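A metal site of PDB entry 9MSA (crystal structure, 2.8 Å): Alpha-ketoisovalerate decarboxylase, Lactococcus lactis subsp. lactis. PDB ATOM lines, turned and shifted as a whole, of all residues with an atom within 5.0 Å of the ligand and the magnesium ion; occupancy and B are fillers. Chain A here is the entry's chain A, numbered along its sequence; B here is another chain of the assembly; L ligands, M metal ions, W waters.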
ATOM      1  N   TYR A  54     -14.882 -24.430 -28.221  1.00  0.00           N
ATOM      2  CA  TYR A  54     -14.764 -23.064 -28.704  1.00  0.00           C
ATOM      3  C   TYR A  54     -15.904 -22.778 -29.680  1.00  0.00           C
ATOM      4  O   TYR A  54     -16.457 -21.683 -29.680  1.00  0.00           O
ATOM      5  CB  TYR A  54     -13.474 -22.916 -29.486  1.00  0.00           C
ATOM      6  CG  TYR A  54     -12.153 -22.838 -28.727  1.00  0.00           C
ATOM      7  CD1 TYR A  54     -12.083 -22.556 -27.359  1.00  0.00           C
ATOM      8  CD2 TYR A  54     -10.955 -22.994 -29.403  1.00  0.00           C
ATOM      9  CE1 TYR A  54     -10.872 -22.425 -26.710  1.00  0.00           C
ATOM     10  CE2 TYR A  54      -9.732 -22.873 -28.761  1.00  0.00           C
ATOM     11  CZ  TYR A  54      -9.681 -22.609 -27.403  1.00  0.00           C
ATOM     12  OH  TYR A  54      -8.451 -22.521 -26.837  1.00  0.00           O
ATOM     13  N   GLN A 377      -7.311 -12.158 -30.005  1.00  0.00           N
ATOM     14  CA  GLN A 377      -6.360 -11.409 -29.188  1.00  0.00           C
ATOM     15  C   GLN A 377      -5.074 -11.224 -29.994  1.00  0.00           C
ATOM     16  O   GLN A 377      -4.669 -12.118 -30.723  1.00  0.00           O
ATOM     17  CB  GLN A 377      -6.071 -12.076 -27.849  1.00  0.00           C
ATOM     18  CG  GLN A 377      -7.270 -12.177 -26.919  1.00  0.00           C
ATOM     19  CD  GLN A 377      -7.957 -10.854 -26.625  1.00  0.00           C
ATOM     20  OE1 GLN A 377      -7.426  -9.980 -25.941  1.00  0.00           O
ATOM     21  NE2 GLN A 377      -9.178 -10.733 -27.132  1.00  0.00           N
ATOM     22  N   GLY A 378      -4.442 -10.056 -29.838  1.00  0.00           N
ATOM     23  CA  GLY A 378      -3.299  -9.655 -30.649  1.00  0.00           C
ATOM     24  C   GLY A 378      -3.722  -8.444 -31.463  1.00  0.00           C
ATOM     25  O   GLY A 378      -4.763  -7.854 -31.172  1.00  0.00           O
ATOM     26  N   THR A 379      -2.919  -8.096 -32.474  1.00  0.00           N
ATOM     27  CA  THR A 379      -3.131  -6.885 -33.272  1.00  0.00           C
ATOM     28  C   THR A 379      -4.593  -6.790 -33.703  1.00  0.00           C
ATOM     29  O   THR A 379      -5.178  -5.707 -33.655  1.00  0.00           O
ATOM     30  CB  THR A 379      -2.172  -6.818 -34.453  1.00  0.00           C
ATOM     31  OG1 THR A 379      -2.403  -7.920 -35.326  1.00  0.00           O
ATOM     32  CG2 THR A 379      -0.716  -6.792 -34.036  1.00  0.00           C
ATOM     33  N   SER A 380      -5.179  -7.928 -34.073  1.00  0.00           N
ATOM     34  CA  SER A 380      -6.532  -8.010 -34.613  1.00  0.00           C
ATOM     35  C   SER A 380      -7.569  -7.444 -33.645  1.00  0.00           C
ATOM     36  O   SER A 380      -8.355  -6.587 -34.020  1.00  0.00           O
ATOM     37  CB  SER A 380      -6.891  -9.406 -35.048  1.00  0.00           C
ATOM     38  OG  SER A 380      -5.838 -10.017 -35.789  1.00  0.00           O
ATOM     39  N   GLY A 402      -9.218 -14.826 -23.060  1.00  0.00           N
ATOM     40  CA  GLY A 402      -8.049 -14.439 -23.830  1.00  0.00           C
ATOM     41  C   GLY A 402      -7.295 -15.649 -24.334  1.00  0.00           C
ATOM     42  O   GLY A 402      -6.065 -15.632 -24.351  1.00  0.00           O
ATOM     43  N   SER A 403      -8.024 -16.689 -24.731  1.00  0.00           N
ATOM     44  CA  SER A 403      -7.423 -17.922 -25.198  1.00  0.00           C
ATOM     45  C   SER A 403      -7.213 -17.826 -26.710  1.00  0.00           C
ATOM     46  O   SER A 403      -8.196 -17.777 -27.458  1.00  0.00           O
ATOM     47  CB  SER A 403      -8.315 -19.068 -24.818  1.00  0.00           C
ATOM     48  OG  SER A 403      -7.863 -20.286 -25.414  1.00  0.00           O
ATOM     49  N   ILE A 404      -5.953 -17.818 -27.177  1.00  0.00           N
ATOM     50  CA  ILE A 404      -5.713 -17.657 -28.604  1.00  0.00           C
ATOM     51  C   ILE A 404      -6.070 -18.935 -29.361  1.00  0.00           C
ATOM     52  O   ILE A 404      -5.869 -20.054 -28.890  1.00  0.00           O
ATOM     53  CB  ILE A 404      -4.289 -17.174 -28.915  1.00  0.00           C
ATOM     54  CG1 ILE A 404      -3.233 -18.144 -28.487  1.00  0.00           C
ATOM     55  CG2 ILE A 404      -4.013 -15.788 -28.355  1.00  0.00           C
ATOM     56  CD1 ILE A 404      -1.879 -17.768 -29.042  1.00  0.00           C
ATOM     57  N   GLY A 428      -4.776 -13.799 -36.162  1.00  0.00           N
ATOM     58  CA  GLY A 428      -3.350 -13.706 -36.434  1.00  0.00           C
ATOM     59  C   GLY A 428      -2.795 -15.087 -36.790  1.00  0.00           C
ATOM     60  O   GLY A 428      -3.367 -16.123 -36.432  1.00  0.00           O
ATOM     61  N   ASP A 429      -1.658 -15.083 -37.509  1.00  0.00           N
ATOM     62  CA  ASP A 429      -0.940 -16.289 -37.903  1.00  0.00           C
ATOM     63  C   ASP A 429      -0.670 -17.172 -36.676  1.00  0.00           C
ATOM     64  O   ASP A 429      -0.940 -18.379 -36.684  1.00  0.00           O
ATOM     65  CB  ASP A 429       0.292 -15.911 -38.701  1.00  0.00           C
ATOM     66  CG  ASP A 429       1.309 -14.993 -38.035  1.00  0.00           C
ATOM     67  OD1 ASP A 429       0.921 -14.287 -37.073  1.00  0.00           O
ATOM     68  OD2 ASP A 429       2.494 -15.021 -38.468  1.00  0.00           O
ATOM     69  N   GLY A 430      -0.176 -16.553 -35.604  1.00  0.00           N
ATOM     70  CA  GLY A 430       0.136 -17.244 -34.372  1.00  0.00           C
ATOM     71  C   GLY A 430      -1.054 -18.035 -33.870  1.00  0.00           C
ATOM     72  O   GLY A 430      -0.914 -19.197 -33.529  1.00  0.00           O
ATOM     73  N   SER A 431      -2.229 -17.404 -33.834  1.00  0.00           N
ATOM     74  CA  SER A 431      -3.425 -17.989 -33.258  1.00  0.00           C
ATOM     75  C   SER A 431      -4.016 -19.075 -34.145  1.00  0.00           C
ATOM     76  O   SER A 431      -4.499 -20.070 -33.648  1.00  0.00           O
ATOM     77  CB  SER A 431      -4.460 -16.947 -32.975  1.00  0.00           C
ATOM     78  OG  SER A 431      -4.006 -16.026 -32.012  1.00  0.00           O
ATOM     79  N   LEU A 434      -3.397 -22.764 -33.667  1.00  0.00           N
ATOM     80  CA  LEU A 434      -3.924 -23.546 -32.561  1.00  0.00           C
ATOM     81  C   LEU A 434      -5.131 -24.373 -33.018  1.00  0.00           C
ATOM     82  O   LEU A 434      -5.364 -25.445 -32.475  1.00  0.00           O
ATOM     83  CB  LEU A 434      -4.244 -22.735 -31.307  1.00  0.00           C
ATOM     84  CG  LEU A 434      -3.034 -22.286 -30.475  1.00  0.00           C
ATOM     85  CD1 LEU A 434      -2.477 -20.971 -30.967  1.00  0.00           C
ATOM     86  CD2 LEU A 434      -3.370 -22.193 -28.989  1.00  0.00           C
ATOM     87  N   ILE A 454      -3.883 -12.546 -40.375  1.00  0.00           N
ATOM     88  CA  ILE A 454      -2.914 -11.464 -40.335  1.00  0.00           C
ATOM     89  C   ILE A 454      -1.525 -12.049 -40.112  1.00  0.00           C
ATOM     90  O   ILE A 454      -1.149 -12.375 -38.984  1.00  0.00           O
ATOM     91  CB  ILE A 454      -3.318 -10.412 -39.301  1.00  0.00           C
ATOM     92  CG1 ILE A 454      -4.684  -9.857 -39.639  1.00  0.00           C
ATOM     93  CG2 ILE A 454      -2.250  -9.311 -39.205  1.00  0.00           C
ATOM     94  CD1 ILE A 454      -5.259  -8.935 -38.593  1.00  0.00           C
ATOM     95  N   ASN A 456       2.048 -11.618 -39.826  1.00  0.00           N
ATOM     96  CA  ASN A 456       3.053 -10.668 -39.367  1.00  0.00           C
ATOM     97  C   ASN A 456       4.206 -11.457 -38.769  1.00  0.00           C
ATOM     98  O   ASN A 456       4.929 -10.970 -37.887  1.00  0.00           O
ATOM     99  CB  ASN A 456       2.450  -9.633 -38.422  1.00  0.00           C
ATOM    100  CG  ASN A 456       1.728 -10.202 -37.228  1.00  0.00           C
ATOM    101  OD1 ASN A 456       1.821 -11.404 -36.926  1.00  0.00           O
ATOM    102  ND2 ASN A 456       0.997  -9.355 -36.527  1.00  0.00           N
ATOM    103  N   GLY A 458       4.745 -14.105 -36.790  1.00  0.00           N
ATOM    104  CA  GLY A 458       4.909 -14.368 -35.372  1.00  0.00           C
ATOM    105  C   GLY A 458       3.843 -13.719 -34.487  1.00  0.00           C
ATOM    106  O   GLY A 458       2.788 -13.289 -34.961  1.00  0.00           O
ATOM    107  N   TYR A 459       4.145 -13.731 -33.186  1.00  0.00           N
ATOM    108  CA  TYR A 459       3.323 -13.177 -32.125  1.00  0.00           C
ATOM    109  C   TYR A 459       3.743 -11.721 -31.890  1.00  0.00           C
ATOM    110  O   TYR A 459       4.622 -11.456 -31.060  1.00  0.00           O
ATOM    111  CB  TYR A 459       3.707 -13.988 -30.888  1.00  0.00           C
ATOM    112  CG  TYR A 459       3.456 -15.489 -30.848  1.00  0.00           C
ATOM    113  CD1 TYR A 459       2.355 -16.048 -31.475  1.00  0.00           C
ATOM    114  CD2 TYR A 459       4.299 -16.342 -30.129  1.00  0.00           C
ATOM    115  CE1 TYR A 459       2.102 -17.413 -31.400  1.00  0.00           C
ATOM    116  CE2 TYR A 459       4.049 -17.697 -30.037  1.00  0.00           C
ATOM    117  CZ  TYR A 459       2.952 -18.238 -30.687  1.00  0.00           C
ATOM    118  OH  TYR A 459       2.678 -19.572 -30.652  1.00  0.00           O
ATOM    119  N   THR A 460       3.126 -10.781 -32.626  1.00  0.00           N
ATOM    120  CA  THR A 460       3.498  -9.376 -32.554  1.00  0.00           C
ATOM    121  C   THR A 460       3.158  -8.811 -31.181  1.00  0.00           C
ATOM    122  O   THR A 460       3.998  -8.131 -30.578  1.00  0.00           O
ATOM    123  CB  THR A 460       2.874  -8.586 -33.706  1.00  0.00           C
ATOM    124  OG1 THR A 460       3.779  -8.845 -34.772  1.00  0.00           O
ATOM    125  CG2 THR A 460       2.884  -7.080 -33.477  1.00  0.00           C
ATOM    126  N   VAL A 461       1.956  -9.104 -30.677  1.00  0.00           N
ATOM    127  CA  VAL A 461       1.522  -8.571 -29.389  1.00  0.00           C
ATOM    128  C   VAL A 461       2.531  -8.936 -28.309  1.00  0.00           C
ATOM    129  O   VAL A 461       2.855  -8.101 -27.463  1.00  0.00           O
ATOM    130  CB  VAL A 461       0.087  -8.954 -28.996  1.00  0.00           C
ATOM    131  CG1 VAL A 461      -0.057 -10.458 -28.721  1.00  0.00           C
ATOM    132  CG2 VAL A 461      -0.403  -8.181 -27.788  1.00  0.00           C
ATOM    133  N   GLU A 462       3.021 -10.193 -28.329  1.00  0.00           N
ATOM    134  CA  GLU A 462       4.036 -10.654 -27.392  1.00  0.00           C
ATOM    135  C   GLU A 462       5.309  -9.841 -27.576  1.00  0.00           C
ATOM    136  O   GLU A 462       5.911  -9.430 -26.593  1.00  0.00           O
ATOM    137  CB  GLU A 462       4.396 -12.140 -27.524  1.00  0.00           C
ATOM    138  CG  GLU A 462       3.229 -13.105 -27.345  1.00  0.00           C
ATOM    139  CD  GLU A 462       2.499 -13.017 -26.022  1.00  0.00           C
ATOM    140  OE1 GLU A 462       2.545 -14.053 -25.354  1.00  0.00           O
ATOM    141  OE2 GLU A 462       1.903 -11.966 -25.657  1.00  0.00           O
ATOM    142  N   VAL B  23       4.252 -23.103 -24.942  1.00  0.00           N
ATOM    143  CA  VAL B  23       3.724 -21.987 -25.717  1.00  0.00           C
ATOM    144  C   VAL B  23       3.868 -20.712 -24.879  1.00  0.00           C
ATOM    145  O   VAL B  23       3.418 -20.674 -23.733  1.00  0.00           O
ATOM    146  CB  VAL B  23       2.251 -22.194 -26.126  1.00  0.00           C
ATOM    147  CG1 VAL B  23       1.661 -20.976 -26.824  1.00  0.00           C
ATOM    148  CG2 VAL B  23       2.033 -23.475 -26.925  1.00  0.00           C
ATOM    149  N   PRO B  24       4.466 -19.637 -25.431  1.00  0.00           N
ATOM    150  CA  PRO B  24       4.645 -18.397 -24.683  1.00  0.00           C
ATOM    151  C   PRO B  24       3.329 -17.741 -24.321  1.00  0.00           C
ATOM    152  O   PRO B  24       2.351 -17.873 -25.040  1.00  0.00           O
ATOM    153  CB  PRO B  24       5.362 -17.468 -25.636  1.00  0.00           C
ATOM    154  CG  PRO B  24       5.944 -18.392 -26.670  1.00  0.00           C
ATOM    155  CD  PRO B  24       5.024 -19.572 -26.787  1.00  0.00           C
ATOM    156  N   GLY B  25       3.345 -17.045 -23.189  1.00  0.00           N
ATOM    157  CA  GLY B  25       2.298 -16.106 -22.830  1.00  0.00           C
ATOM    158  C   GLY B  25       2.906 -14.984 -22.002  1.00  0.00           C
ATOM    159  O   GLY B  25       4.041 -15.099 -21.545  1.00  0.00           O
ATOM    160  N   ASP B  26       2.147 -13.919 -21.799  1.00  0.00           N
ATOM    161  CA  ASP B  26       2.693 -12.757 -21.117  1.00  0.00           C
ATOM    162  C   ASP B  26       3.236 -13.139 -19.731  1.00  0.00           C
ATOM    163  O   ASP B  26       4.255 -12.595 -19.332  1.00  0.00           O
ATOM    164  CB  ASP B  26       1.736 -11.587 -21.162  1.00  0.00           C
ATOM    165  CG  ASP B  26       0.422 -11.832 -20.458  1.00  0.00           C
ATOM    166  OD1 ASP B  26      -0.254 -12.860 -20.776  1.00  0.00           O
ATOM    167  OD2 ASP B  26       0.091 -10.987 -19.591  1.00  0.00           O
ATOM    168  N   GLU B  49      -0.819 -25.783 -26.636  1.00  0.00           N
ATOM    169  CA  GLU B  49      -0.390 -26.333 -25.366  1.00  0.00           C
ATOM    170  C   GLU B  49      -0.678 -27.833 -25.273  1.00  0.00           C
ATOM    171  O   GLU B  49       0.154 -28.566 -24.744  1.00  0.00           O
ATOM    172  CB  GLU B  49      -1.035 -25.597 -24.195  1.00  0.00           C
ATOM    173  CG  GLU B  49      -0.482 -24.192 -23.960  1.00  0.00           C
ATOM    174  CD  GLU B  49      -1.065 -23.064 -24.817  1.00  0.00           C
ATOM    175  OE1 GLU B  49      -1.959 -23.300 -25.675  1.00  0.00           O
ATOM    176  OE2 GLU B  49      -0.625 -21.929 -24.589  1.00  0.00           O
ATOM    177  N   THR B  71       1.072 -20.933 -19.974  1.00  0.00           N
ATOM    178  CA  THR B  71       0.675 -19.696 -19.315  1.00  0.00           C
ATOM    179  C   THR B  71      -0.557 -19.983 -18.443  1.00  0.00           C
ATOM    180  O   THR B  71      -1.338 -20.883 -18.753  1.00  0.00           O
ATOM    181  CB  THR B  71       0.437 -18.622 -20.369  1.00  0.00           C
ATOM    182  OG1 THR B  71       0.290 -17.404 -19.653  1.00  0.00           O
ATOM    183  CG2 THR B  71      -0.799 -18.884 -21.217  1.00  0.00           C
ATOM    184  N   VAL B  74      -5.356 -20.321 -19.574  1.00  0.00           N
ATOM    185  CA  VAL B  74      -5.594 -20.775 -20.940  1.00  0.00           C
ATOM    186  C   VAL B  74      -4.573 -21.849 -21.343  1.00  0.00           C
ATOM    187  O   VAL B  74      -4.918 -22.794 -22.035  1.00  0.00           O
ATOM    188  CB  VAL B  74      -5.608 -19.623 -21.945  1.00  0.00           C
ATOM    189  CG1 VAL B  74      -6.753 -18.666 -21.676  1.00  0.00           C
ATOM    190  CG2 VAL B  74      -4.277 -18.896 -22.014  1.00  0.00           C
ATOM    191  N   GLY B  75      -3.321 -21.677 -20.903  1.00  0.00           N
ATOM    192  CA  GLY B  75      -2.280 -22.614 -21.275  1.00  0.00           C
ATOM    193  C   GLY B  75      -2.428 -23.951 -20.534  1.00  0.00           C
ATOM    194  O   GLY B  75      -2.454 -25.016 -21.153  1.00  0.00           O
ATOM    195  N   SER B  78      -5.421 -26.042 -21.341  1.00  0.00           N
ATOM    196  CA  SER B  78      -5.365 -26.657 -22.652  1.00  0.00           C
ATOM    197  C   SER B  78      -4.611 -27.992 -22.569  1.00  0.00           C
ATOM    198  O   SER B  78      -4.953 -28.954 -23.274  1.00  0.00           O
ATOM    199  CB  SER B  78      -4.738 -25.739 -23.656  1.00  0.00           C
ATOM    200  OG  SER B  78      -5.587 -24.638 -23.936  1.00  0.00           O
ATOM    201  N   HIS B 113      -7.076 -14.259 -18.424  1.00  0.00           N
ATOM    202  CA  HIS B 113      -6.859 -15.665 -18.146  1.00  0.00           C
ATOM    203  C   HIS B 113      -7.376 -16.028 -16.754  1.00  0.00           C
ATOM    204  O   HIS B 113      -6.885 -16.977 -16.148  1.00  0.00           O
ATOM    205  CB  HIS B 113      -5.395 -16.085 -18.355  1.00  0.00           C
ATOM    206  CG  HIS B 113      -4.770 -15.753 -19.673  1.00  0.00           C
ATOM    207  ND1 HIS B 113      -5.441 -15.323 -20.786  1.00  0.00           N
ATOM    208  CD2 HIS B 113      -3.461 -15.782 -20.018  1.00  0.00           C
ATOM    209  CE1 HIS B 113      -4.571 -15.112 -21.769  1.00  0.00           C
ATOM    210  NE2 HIS B 113      -3.352 -15.385 -21.322  1.00  0.00           N
HETATM  211  N1  LIG L   1      -2.056 -19.603 -25.406  1.00  0.00           N
HETATM  212  C1  LIG L   1      -3.354 -19.311 -25.368  1.00  0.00           C
HETATM  213  C2  LIG L   1      -4.331 -20.432 -25.524  1.00  0.00           C
HETATM  214  N2  LIG L   1      -3.860 -18.087 -25.206  1.00  0.00           N
HETATM  215  C3  LIG L   1      -2.978 -17.080 -25.036  1.00  0.00           C
HETATM  216  N3  LIG L   1      -3.485 -15.858 -24.825  1.00  0.00           N
HETATM  217  C4  LIG L   1      -1.579 -17.291 -25.057  1.00  0.00           C
HETATM  218  C5  LIG L   1      -1.171 -18.589 -25.253  1.00  0.00           C
HETATM  219  C6  LIG L   1      -0.605 -16.125 -24.940  1.00  0.00           C
HETATM  220  N4  LIG L   1      -0.750 -15.178 -26.059  1.00  0.00           N
HETATM  221  C7  LIG L   1      -1.662 -14.145 -26.098  1.00  0.00           C
HETATM  222  S1  LIG L   1      -1.647 -13.262 -27.569  1.00  0.00           S
HETATM  223  C8  LIG L   1      -0.401 -14.233 -28.188  1.00  0.00           C
HETATM  224  C9  LIG L   1      -0.019 -15.230 -27.262  1.00  0.00           C
HETATM  225  C10 LIG L   1       1.042 -16.257 -27.499  1.00  0.00           C
HETATM  226  C11 LIG L   1       0.193 -13.970 -29.518  1.00  0.00           C
HETATM  227  C12 LIG L   1      -0.810 -13.868 -30.602  1.00  0.00           C
HETATM  228  O1  LIG L   1      -0.058 -13.781 -31.847  1.00  0.00           O
HETATM  229  P1  LIG L   1      -0.819 -13.654 -33.245  1.00  0.00           P
HETATM  230  O2  LIG L   1       0.208 -13.835 -34.330  1.00  0.00           O
HETATM  231  O3  LIG L   1      -2.082 -14.460 -33.245  1.00  0.00           O
HETATM  232  O4  LIG L   1      -1.211 -12.098 -33.139  1.00  0.00           O
HETATM  233  P2  LIG L   1      -0.476 -10.799 -33.732  1.00  0.00           P
HETATM  234  O5  LIG L   1      -0.411  -9.826 -32.565  1.00  0.00           O
HETATM  235  O6  LIG L   1      -1.451 -10.418 -34.827  1.00  0.00           O
HETATM  236  O7  LIG L   1       0.883 -11.237 -34.246  1.00  0.00           O
HETATM  237 MG    MG M   1       0.478 -12.583 -35.902  1.00  0.00          MG
HETATM  238  O   HOH W   1      -0.149 -12.501 -23.892  1.00  0.00           O
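O of Gly 402 lies within hydrogen-bond range of N3 of the ligand, at 2.6 Å. O5 of the ligand sits at hydrogen-bond distance from N of Thr 379 (3.0 Å). An oxygen (O6) of the ligand sits at hydrogen-bond distance from the side-chain hydroxyl of Thr 379 (2.7 Å). N of Ser 431 sits at hydrogen-bond distance from O3 of the ligand, 3.0 Å away. The side-chain hydroxyl of Ser 431 is in hydrogen-bond range of an oxygen (O3) of the ligand (2.8 Å). N of Thr 460 sits close to O7 of the ligand, 2.8 Å away. N1 of the ligand lies within hydrogen-bond range of OE2 of Glu 49 of chain B, 2.9 Å away. The backbone NH (N) of Ile 404 sits at hydrogen-bond distance from a nitrogen (N2) of the ligand. An oxygen (O2) of the ligand lies close to the backbone NH of Gly 430 (3.0 Å). The backbone NH (N) of Val 461 sits at hydrogen-bond distance from an oxygen (O5) of the ligand (3.1 Å).
The side-chain amide nitrogen of Asn 456 is in hydrogen-bond range of the side-chain hydroxyl of Thr 460 (3.3 Å). N of Asp 429 lies within hydrogen-bond range of O of Ile 454 (3.1 Å). OG of Ser 78 of chain B is in hydrogen-bond range of O of Val 74 of chain B. The side-chain hydroxyl of Tyr 54 sits at hydrogen-bond distance from the side-chain hydroxyl of Ser 403 (2.7 Å).
Gly 378 touches the ligand (CA to O5, 3.5 Å). Ser 403 touches the ligand. Gly 428 touches the ligand. Tyr 459 touches the ligand (CD1 to O1, 3.3 Å). Glu 462 touches the ligand. Pro 24 of chain B touches the ligand (O to C10, 3.2 Å). CA of Gly 25 of chain B touches C6 of the ligand, at 3.6 Å. Val 74 of chain B touches the ligand (CG2 to N2, 3.3 Å). His 113 of chain B touches the ligand (CE1 to N3, 3.3 Å). Hydrophobic or aromatic side chains within 4 Å of the ligand: Ile 404, Tyr 459, Val 461, Val 74 of chain B and His 113 of chain B. Within 4 Å of the ligand: Gly 378, Thr 379, Gly 402, Ser 403, Ile 404, Gly 428, Asp 429, Gly 430, Ser 431, Asn 456, Gly 458, Tyr 459, Thr 460, Val 461, Glu 462, Pro 24 of chain B, Gly 25 of chain B, Glu 49 of chain B, Val 74 of chain B and His 113 of chain B. The nearest printed residue that does not touch the ligand is Leu 434 (4.004 Å).
Ile 454 touches the magnesium ion (O to MG, 3.5 Å). The nearest printed residue that does not touch the magnesium ion is Gly 428 (4.02 Å).
The magnesium ion is bound by an oxygen (O2) of the ligand (2.0 Å), the side-chain amide oxygen of Asn 456 (2.1 Å), the side-chain carboxylate of Asp 429 (2.1 Å), an oxygen (O7) of the ligand (2.2 Å) and the backbone carbonyl oxygen of Gly 458 (2.6 Å).
Water W1 lies within hydrogen-bond range of OE2 of Glu 462 (2.8 Å) and OD1 of Asp 26 of chain B (3.1 Å).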
